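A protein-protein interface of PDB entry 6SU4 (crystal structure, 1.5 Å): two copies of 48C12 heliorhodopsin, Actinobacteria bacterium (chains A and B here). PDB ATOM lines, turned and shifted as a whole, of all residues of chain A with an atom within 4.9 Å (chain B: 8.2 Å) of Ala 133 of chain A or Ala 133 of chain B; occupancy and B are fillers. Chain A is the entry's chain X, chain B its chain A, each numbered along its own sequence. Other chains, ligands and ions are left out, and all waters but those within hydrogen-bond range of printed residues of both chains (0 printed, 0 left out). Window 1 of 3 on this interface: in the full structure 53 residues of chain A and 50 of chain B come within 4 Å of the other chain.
Hydrophobic or aromatic side chains of chain B within 4 Å of the printed part of chain A: Val 129, Ala 130, Leu 132, Ala 133, Ile 134, Val 137 and Val 171. Hydrophobic or aromatic side chains of chain A within 4 Å of the printed part of chain B: Val 129, Ala 130, Leu 132, Ala 133, Ile 134, Val 137 and Val 171. Among the printed residues, no Asp or Glu carboxylate lies within 4 Å of a Lys or Arg side-chain nitrogen of the other chain.
CG1 of Val 129 of chain A touches CD1 of Ile 134 of chain B (3.7 Å). Gly 175 of chain B touches Val 129 of chain A. Ala 130 of chain A touches Asp 127 of chain B. Leu 132 of chain A touches Gly 175 of chain B. Ala 133 of chain B touches Ala 133 of chain A (CB to CB, 3.4 Å). Ile 134 of chain A touches Ala 133 of chain B. Gly 136 of chain A touches Val 137 of chain B (C to CG2, 3.7 Å). N of Val 137 of chain A touches CG2 of Val 137 of chain B (3.8 Å). O of Val 171 of chain A touches CD2 of Leu 132 of chain B, at 3.7 Å. Val 171 of chain A touches Ala 133 of chain B.
Val 129 of chain A touches Ile 134 of chain B, and with the chains exchanged Ile 134 of chain A touches Val 129 of chain B. Leu 132 of chain A touches Val 171 of chain B, and with the chains exchanged Val 171 of chain A touches Leu 132 of chain B. Ala 133 of chain B touches its own counterpart, Ala 133 of chain A. Ala 133 of chain A touches Val 171 of chain B, and with the chains exchanged Val 171 of chain A touches Ala 133 of chain B. Positions printed for both chains: 129, 130, 131, 132, 133, 134, 135, 136, 137, 138 and 171.
Of the printed residues of chain B, Leu 132 of chain A touches Val 171 and Gly 175. Of chain B, only Ala 133 (3.4 Å), Ile 134 (3.8 Å) and Val 171 (3.9 Å) come within 4 Å of Ala 133 of chain A. Of the printed residues of chain B, Ile 134 of chain A touches Val 129 (3.7 Å) and Ala 133 (3.9 Å). Ala 133 of chain B touches three residues of chain A. Of the printed residues of chain A, Val 171 of chain B touches Leu 132 (3.7 Å) and Ala 133 (3.9 Å). The nearest printed residue of chain B that does not touch Ala 133 of chain A is Ala 130 of chain B (4.4 Å). The nearest printed residue of chain A that does not touch Ala 133 of chain B is Ala 130 of chain A (4.4 Å). The nearest printed residue of chain A that does not touch Ile 134 of chain B is Val 171 of chain A (6.1 Å).
The side-chain carboxylate (OD1) of Asp 127 of chain B lies within hydrogen-bond range of the backbone NH (N) of Val 129 of chain B, at 3.0 Å. The backbone NH (N) of Ala 130 of chain B sits at hydrogen-bond distance from the side-chain carboxylate (OD1) of Asp 127 of chain B, 3.2 Å away. O of Gly 136 of chain B lies within hydrogen-bond range of OG of Ser 140 of chain B.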
ATOM      1  N   VAL A 129      -4.592  -1.751   5.894  1.00  0.00           N
ATOM      2  CA  VAL A 129      -4.631  -3.213   6.174  1.00  0.00           C
ATOM      3  C   VAL A 129      -6.056  -3.585   6.600  1.00  0.00           C
ATOM      4  O   VAL A 129      -6.509  -4.671   6.228  1.00  0.00           O
ATOM      5  CB  VAL A 129      -3.577  -3.646   7.203  1.00  0.00           C
ATOM      6  CG1 VAL A 129      -3.718  -5.123   7.534  1.00  0.00           C
ATOM      7  CG2 VAL A 129      -2.176  -3.328   6.699  1.00  0.00           C
ATOM      8  N   ALA A 130      -6.752  -2.715   7.331  1.00  0.00           N
ATOM      9  CA  ALA A 130      -8.179  -2.933   7.658  1.00  0.00           C
ATOM     10  C   ALA A 130      -8.948  -3.102   6.347  1.00  0.00           C
ATOM     11  O   ALA A 130      -9.750  -4.038   6.230  1.00  0.00           O
ATOM     12  CB  ALA A 130      -8.725  -1.800   8.481  1.00  0.00           C
ATOM     13  N   LEU A 131      -8.726  -2.210   5.385  1.00  0.00           N
ATOM     14  CA  LEU A 131      -9.522  -2.234   4.128  1.00  0.00           C
ATOM     15  C   LEU A 131      -9.124  -3.445   3.277  1.00  0.00           C
ATOM     16  O   LEU A 131     -10.020  -4.122   2.740  1.00  0.00           O
ATOM     17  CB  LEU A 131      -9.340  -0.908   3.399  1.00  0.00           C
ATOM     18  CG  LEU A 131      -9.777   0.308   4.213  1.00  0.00           C
ATOM     19  CD1 LEU A 131      -9.471   1.592   3.463  1.00  0.00           C
ATOM     20  CD2 LEU A 131     -11.260   0.229   4.573  1.00  0.00           C
ATOM     21  N   LEU A 132      -7.830  -3.738   3.168  1.00  0.00           N
ATOM     22  CA  LEU A 132      -7.347  -4.927   2.429  1.00  0.00           C
ATOM     23  C   LEU A 132      -7.956  -6.196   3.049  1.00  0.00           C
ATOM     24  O   LEU A 132      -8.457  -7.052   2.303  1.00  0.00           O
ATOM     25  CB  LEU A 132      -5.818  -4.955   2.480  1.00  0.00           C
ATOM     26  CG  LEU A 132      -5.188  -6.238   1.953  1.00  0.00           C
ATOM     27  CD1 LEU A 132      -5.399  -6.350   0.453  1.00  0.00           C
ATOM     28  CD2 LEU A 132      -3.702  -6.299   2.299  1.00  0.00           C
ATOM     29  N   ALA A 133      -7.910  -6.343   4.373  1.00  0.00           N
ATOM     30  CA  ALA A 133      -8.367  -7.578   5.044  1.00  0.00           C
ATOM     31  C   ALA A 133      -9.901  -7.654   4.989  1.00  0.00           C
ATOM     32  O   ALA A 133     -10.440  -8.767   4.912  1.00  0.00           O
ATOM     33  CB  ALA A 133      -7.823  -7.634   6.448  1.00  0.00           C
ATOM     34  N   ILE A 134     -10.601  -6.519   5.018  1.00  0.00           N
ATOM     35  CA  ILE A 134     -12.077  -6.514   4.806  1.00  0.00           C
ATOM     36  C   ILE A 134     -12.352  -7.030   3.389  1.00  0.00           C
ATOM     37  O   ILE A 134     -13.243  -7.868   3.224  1.00  0.00           O
ATOM     38  CB  ILE A 134     -12.682  -5.117   5.039  1.00  0.00           C
ATOM     39  CG1 ILE A 134     -12.792  -4.813   6.536  1.00  0.00           C
ATOM     40  CG2 ILE A 134     -14.024  -5.004   4.331  1.00  0.00           C
ATOM     41  CD1 ILE A 134     -13.060  -3.356   6.842  1.00  0.00           C
ATOM     42  N   PHE A 135     -11.605  -6.554   2.392  1.00  0.00           N
ATOM     43  CA  PHE A 135     -11.785  -7.003   0.993  1.00  0.00           C
ATOM     44  C   PHE A 135     -11.587  -8.524   0.954  1.00  0.00           C
ATOM     45  O   PHE A 135     -12.445  -9.235   0.414  1.00  0.00           O
ATOM     46  CB  PHE A 135     -10.832  -6.265   0.045  1.00  0.00           C
ATOM     47  CG  PHE A 135     -11.145  -6.466  -1.413  1.00  0.00           C
ATOM     48  CD1 PHE A 135     -11.767  -5.465  -2.137  1.00  0.00           C
ATOM     49  CD2 PHE A 135     -10.850  -7.663  -2.049  1.00  0.00           C
ATOM     50  CE1 PHE A 135     -12.075  -5.646  -3.475  1.00  0.00           C
ATOM     51  CE2 PHE A 135     -11.169  -7.844  -3.385  1.00  0.00           C
ATOM     52  CZ  PHE A 135     -11.782  -6.837  -4.092  1.00  0.00           C
ATOM     53  N   GLY A 136     -10.492  -9.010   1.540  1.00  0.00           N
ATOM     54  CA  GLY A 136     -10.122 -10.436   1.550  1.00  0.00           C
ATOM     55  C   GLY A 136     -11.154 -11.316   2.238  1.00  0.00           C
ATOM     56  O   GLY A 136     -11.475 -12.380   1.690  1.00  0.00           O
ATOM     57  N   VAL A 137     -11.645 -10.916   3.409  1.00  0.00           N
ATOM     58  CA  VAL A 137     -12.571 -11.776   4.204  1.00  0.00           C
ATOM     59  C   VAL A 137     -13.945 -11.742   3.530  1.00  0.00           C
ATOM     60  O   VAL A 137     -14.656 -12.765   3.550  1.00  0.00           O
ATOM     61  CB  VAL A 137     -12.624 -11.390   5.691  1.00  0.00           C
ATOM     62  CG1 VAL A 137     -13.400 -10.110   5.961  1.00  0.00           C
ATOM     63  CG2 VAL A 137     -13.186 -12.531   6.527  1.00  0.00           C
ATOM     64  N   ASN A 138     -14.320 -10.607   2.938  1.00  0.00           N
ATOM     65  CA  ASN A 138     -15.591 -10.515   2.175  1.00  0.00           C
ATOM     66  C   ASN A 138     -15.501 -11.389   0.918  1.00  0.00           C
ATOM     67  O   ASN A 138     -16.455 -12.145   0.631  1.00  0.00           O
ATOM     68  CB  ASN A 138     -15.931  -9.075   1.798  1.00  0.00           C
ATOM     69  CG  ASN A 138     -17.316  -8.986   1.197  1.00  0.00           C
ATOM     70  OD1 ASN A 138     -18.309  -8.901   1.920  1.00  0.00           O
ATOM     71  ND2 ASN A 138     -17.389  -9.038  -0.124  1.00  0.00           N
ATOM     72  N   VAL A 171     -17.653 -10.662   9.570  1.00  0.00           N
ATOM     73  CA  VAL A 171     -16.457  -9.983  10.141  1.00  0.00           C
ATOM     74  C   VAL A 171     -16.445  -8.499   9.773  1.00  0.00           C
ATOM     75  O   VAL A 171     -16.284  -7.663  10.654  1.00  0.00           O
ATOM     76  CB  VAL A 171     -15.161 -10.710   9.739  1.00  0.00           C
ATOM     77  CG1 VAL A 171     -13.938  -9.861  10.041  1.00  0.00           C
ATOM     78  CG2 VAL A 171     -15.080 -12.062  10.424  1.00  0.00           C
ATOM     79  N   ILE B 116      -0.962 -14.808  13.756  1.00  0.00           N
ATOM     80  CA  ILE B 116      -0.801 -13.777  12.693  1.00  0.00           C
ATOM     81  C   ILE B 116      -1.249 -12.418  13.238  1.00  0.00           C
ATOM     82  O   ILE B 116      -0.614 -11.395  12.881  1.00  0.00           O
ATOM     83  CB  ILE B 116      -1.496 -14.209  11.383  1.00  0.00           C
ATOM     84  CG1 ILE B 116      -1.117 -13.283  10.225  1.00  0.00           C
ATOM     85  CG2 ILE B 116      -3.000 -14.326  11.544  1.00  0.00           C
ATOM     86  CD1 ILE B 116       0.367 -13.185   9.971  1.00  0.00           C
ATOM     87  N   VAL B 117      -2.240 -12.376  14.135  1.00  0.00           N
ATOM     88  CA  VAL B 117      -2.622 -11.088  14.778  1.00  0.00           C
ATOM     89  C   VAL B 117      -1.424 -10.581  15.592  1.00  0.00           C
ATOM     90  O   VAL B 117      -1.126  -9.388  15.515  1.00  0.00           O
ATOM     91  CB  VAL B 117      -3.894 -11.202  15.632  1.00  0.00           C
ATOM     92  CG1 VAL B 117      -4.070  -9.974  16.500  1.00  0.00           C
ATOM     93  CG2 VAL B 117      -5.118 -11.437  14.770  1.00  0.00           C
ATOM     94  N   ASP B 127      -4.873  -0.902  14.271  1.00  0.00           N
ATOM     95  CA  ASP B 127      -6.315  -0.642  14.046  1.00  0.00           C
ATOM     96  C   ASP B 127      -7.104  -1.914  14.372  1.00  0.00           C
ATOM     97  O   ASP B 127      -6.769  -2.992  13.845  1.00  0.00           O
ATOM     98  CB  ASP B 127      -6.596  -0.181  12.622  1.00  0.00           C
ATOM     99  CG  ASP B 127      -8.054   0.184  12.470  1.00  0.00           C
ATOM    100  OD1 ASP B 127      -8.842  -0.715  12.120  1.00  0.00           O
ATOM    101  OD2 ASP B 127      -8.389   1.357  12.753  1.00  0.00           O
ATOM    102  N   ILE B 128      -8.134  -1.803  15.206  1.00  0.00           N
ATOM    103  CA  ILE B 128      -8.847  -2.992  15.750  1.00  0.00           C
ATOM    104  C   ILE B 128      -9.537  -3.733  14.599  1.00  0.00           C
ATOM    105  O   ILE B 128      -9.624  -4.973  14.645  1.00  0.00           O
ATOM    106  CB  ILE B 128      -9.807  -2.588  16.886  1.00  0.00           C
ATOM    107  CG1 ILE B 128     -10.353  -3.819  17.610  1.00  0.00           C
ATOM    108  CG2 ILE B 128     -10.914  -1.671  16.391  1.00  0.00           C
ATOM    109  CD1 ILE B 128     -10.987  -3.506  18.950  1.00  0.00           C
ATOM    110  N   VAL B 129     -10.011  -3.013  13.588  1.00  0.00           N
ATOM    111  CA  VAL B 129     -10.677  -3.654  12.425  1.00  0.00           C
ATOM    112  C   VAL B 129      -9.617  -4.361  11.577  1.00  0.00           C
ATOM    113  O   VAL B 129      -9.905  -5.476  11.108  1.00  0.00           O
ATOM    114  CB  VAL B 129     -11.521  -2.653  11.620  1.00  0.00           C
ATOM    115  CG1 VAL B 129     -12.160  -3.346  10.428  1.00  0.00           C
ATOM    116  CG2 VAL B 129     -12.579  -1.997  12.495  1.00  0.00           C
ATOM    117  N   ALA B 130      -8.423  -3.784  11.419  1.00  0.00           N
ATOM    118  CA  ALA B 130      -7.304  -4.472  10.734  1.00  0.00           C
ATOM    119  C   ALA B 130      -7.063  -5.823  11.415  1.00  0.00           C
ATOM    120  O   ALA B 130      -6.951  -6.837  10.722  1.00  0.00           O
ATOM    121  CB  ALA B 130      -6.049  -3.631  10.753  1.00  0.00           C
ATOM    122  N   LEU B 131      -6.973  -5.844  12.740  1.00  0.00           N
ATOM    123  CA  LEU B 131      -6.603  -7.080  13.475  1.00  0.00           C
ATOM    124  C   LEU B 131      -7.775  -8.070  13.443  1.00  0.00           C
ATOM    125  O   LEU B 131      -7.544  -9.273  13.262  1.00  0.00           O
ATOM    126  CB  LEU B 131      -6.186  -6.700  14.894  1.00  0.00           C
ATOM    127  CG  LEU B 131      -4.981  -5.758  14.962  1.00  0.00           C
ATOM    128  CD1 LEU B 131      -4.668  -5.376  16.398  1.00  0.00           C
ATOM    129  CD2 LEU B 131      -3.756  -6.371  14.295  1.00  0.00           C
ATOM    130  N   LEU B 132      -9.006  -7.584  13.564  1.00  0.00           N
ATOM    131  CA  LEU B 132     -10.216  -8.438  13.498  1.00  0.00           C
ATOM    132  C   LEU B 132     -10.302  -9.090  12.113  1.00  0.00           C
ATOM    133  O   LEU B 132     -10.557 -10.309  12.025  1.00  0.00           O
ATOM    134  CB  LEU B 132     -11.446  -7.571  13.758  1.00  0.00           C
ATOM    135  CG  LEU B 132     -12.779  -8.262  13.503  1.00  0.00           C
ATOM    136  CD1 LEU B 132     -13.016  -9.381  14.499  1.00  0.00           C
ATOM    137  CD2 LEU B 132     -13.913  -7.247  13.516  1.00  0.00           C
ATOM    138  N   ALA B 133     -10.112  -8.302  11.052  1.00  0.00           N
ATOM    139  CA  ALA B 133     -10.266  -8.798   9.669  1.00  0.00           C
ATOM    140  C   ALA B 133      -9.091  -9.724   9.318  1.00  0.00           C
ATOM    141  O   ALA B 133      -9.300 -10.717   8.583  1.00  0.00           O
ATOM    142  CB  ALA B 133     -10.407  -7.643   8.722  1.00  0.00           C
ATOM    143  N   ILE B 134      -7.892  -9.433   9.820  1.00  0.00           N
ATOM    144  CA  ILE B 134      -6.745 -10.379   9.680  1.00  0.00           C
ATOM    145  C   ILE B 134      -7.130 -11.710  10.347  1.00  0.00           C
ATOM    146  O   ILE B 134      -6.899 -12.760   9.753  1.00  0.00           O
ATOM    147  CB  ILE B 134      -5.446  -9.791  10.254  1.00  0.00           C
ATOM    148  CG1 ILE B 134      -4.831  -8.755   9.307  1.00  0.00           C
ATOM    149  CG2 ILE B 134      -4.465 -10.905  10.569  1.00  0.00           C
ATOM    150  CD1 ILE B 134      -3.710  -7.953   9.921  1.00  0.00           C
ATOM    151  N   PHE B 135      -7.684 -11.685  11.562  1.00  0.00           N
ATOM    152  CA  PHE B 135      -8.107 -12.926  12.255  1.00  0.00           C
ATOM    153  C   PHE B 135      -9.092 -13.684  11.350  1.00  0.00           C
ATOM    154  O   PHE B 135      -8.916 -14.891  11.119  1.00  0.00           O
ATOM    155  CB  PHE B 135      -8.705 -12.615  13.629  1.00  0.00           C
ATOM    156  CG  PHE B 135      -8.842 -13.820  14.522  1.00  0.00           C
ATOM    157  CD1 PHE B 135      -9.855 -14.739  14.322  1.00  0.00           C
ATOM    158  CD2 PHE B 135      -7.956 -14.028  15.566  1.00  0.00           C
ATOM    159  CE1 PHE B 135      -9.980 -15.848  15.146  1.00  0.00           C
ATOM    160  CE2 PHE B 135      -8.077 -15.140  16.385  1.00  0.00           C
ATOM    161  CZ  PHE B 135      -9.089 -16.044  16.175  1.00  0.00           C
ATOM    162  N   GLY B 136     -10.099 -12.984  10.822  1.00  0.00           N
ATOM    163  CA  GLY B 136     -11.172 -13.586  10.014  1.00  0.00           C
ATOM    164  C   GLY B 136     -10.657 -14.170   8.710  1.00  0.00           C
ATOM    165  O   GLY B 136     -11.100 -15.261   8.343  1.00  0.00           O
ATOM    166  N   VAL B 137      -9.777 -13.464   8.005  1.00  0.00           N
ATOM    167  CA  VAL B 137      -9.305 -13.929   6.671  1.00  0.00           C
ATOM    168  C   VAL B 137      -8.324 -15.091   6.887  1.00  0.00           C
ATOM    169  O   VAL B 137      -8.318 -16.020   6.082  1.00  0.00           O
ATOM    170  CB  VAL B 137      -8.724 -12.781   5.824  1.00  0.00           C
ATOM    171  CG1 VAL B 137      -7.343 -12.340   6.270  1.00  0.00           C
ATOM    172  CG2 VAL B 137      -8.708 -13.160   4.350  1.00  0.00           C
ATOM    173  N   ASN B 138      -7.560 -15.072   7.973  1.00  0.00           N
ATOM    174  CA  ASN B 138      -6.652 -16.194   8.316  1.00  0.00           C
ATOM    175  C   ASN B 138      -7.487 -17.423   8.692  1.00  0.00           C
ATOM    176  O   ASN B 138      -7.169 -18.542   8.236  1.00  0.00           O
ATOM    177  CB  ASN B 138      -5.690 -15.817   9.437  1.00  0.00           C
ATOM    178  CG  ASN B 138      -4.665 -16.906   9.646  1.00  0.00           C
ATOM    179  OD1 ASN B 138      -3.646 -16.931   8.948  1.00  0.00           O
ATOM    180  ND2 ASN B 138      -4.953 -17.819  10.565  1.00  0.00           N
ATOM    181  N   ALA B 139      -8.529 -17.249   9.509  1.00  0.00           N
ATOM    182  CA  ALA B 139      -9.445 -18.362   9.847  1.00  0.00           C
ATOM    183  C   ALA B 139     -10.037 -18.916   8.544  1.00  0.00           C
ATOM    184  O   ALA B 139     -10.152 -20.142   8.407  1.00  0.00           O
ATOM    185  CB  ALA B 139     -10.504 -17.904  10.816  1.00  0.00           C
ATOM    186  N   SER B 140     -10.398 -18.041   7.601  1.00  0.00           N
ATOM    187  CA  SER B 140     -11.014 -18.452   6.315  1.00  0.00           C
ATOM    188  C   SER B 140     -10.032 -19.346   5.553  1.00  0.00           C
ATOM    189  O   SER B 140     -10.457 -20.378   5.036  1.00  0.00           O
ATOM    190  CB  SER B 140     -11.408 -17.261   5.491  1.00  0.00           C
ATOM    191  OG  SER B 140     -12.446 -16.539   6.123  1.00  0.00           O
ATOM    192  N   ALA B 168      -7.049 -16.229   0.431  1.00  0.00           N
ATOM    193  CA  ALA B 168      -7.344 -15.716   1.790  1.00  0.00           C
ATOM    194  C   ALA B 168      -6.041 -15.633   2.603  1.00  0.00           C
ATOM    195  O   ALA B 168      -5.789 -14.595   3.239  1.00  0.00           O
ATOM    196  CB  ALA B 168      -8.367 -16.603   2.468  1.00  0.00           C
ATOM    197  N   VAL B 171      -3.371 -12.660   2.317  1.00  0.00           N
ATOM    198  CA  VAL B 171      -3.833 -11.269   2.591  1.00  0.00           C
ATOM    199  C   VAL B 171      -3.127 -10.684   3.819  1.00  0.00           C
ATOM    200  O   VAL B 171      -2.611  -9.576   3.747  1.00  0.00           O
ATOM    201  CB  VAL B 171      -5.365 -11.209   2.708  1.00  0.00           C
ATOM    202  CG1 VAL B 171      -5.823  -9.884   3.297  1.00  0.00           C
ATOM    203  CG2 VAL B 171      -6.016 -11.465   1.356  1.00  0.00           C
ATOM    204  N   PRO B 172      -3.053 -11.360   4.990  1.00  0.00           N
ATOM    205  CA  PRO B 172      -2.378 -10.757   6.144  1.00  0.00           C
ATOM    206  C   PRO B 172      -0.906 -10.434   5.851  1.00  0.00           C
ATOM    207  O   PRO B 172      -0.395  -9.455   6.343  1.00  0.00           O
ATOM    208  CB  PRO B 172      -2.509 -11.825   7.240  1.00  0.00           C
ATOM    209  CG  PRO B 172      -3.735 -12.606   6.829  1.00  0.00           C
ATOM    210  CD  PRO B 172      -3.675 -12.650   5.314  1.00  0.00           C
ATOM    211  N   GLY B 175      -0.492  -7.382   4.011  1.00  0.00           N
ATOM    212  CA  GLY B 175      -0.648  -6.376   5.082  1.00  0.00           C
ATOM    213  C   GLY B 175       0.666  -6.099   5.800  1.00  0.00           C
ATOM    214  O   GLY B 175       1.030  -4.912   5.924  1.00  0.00           O
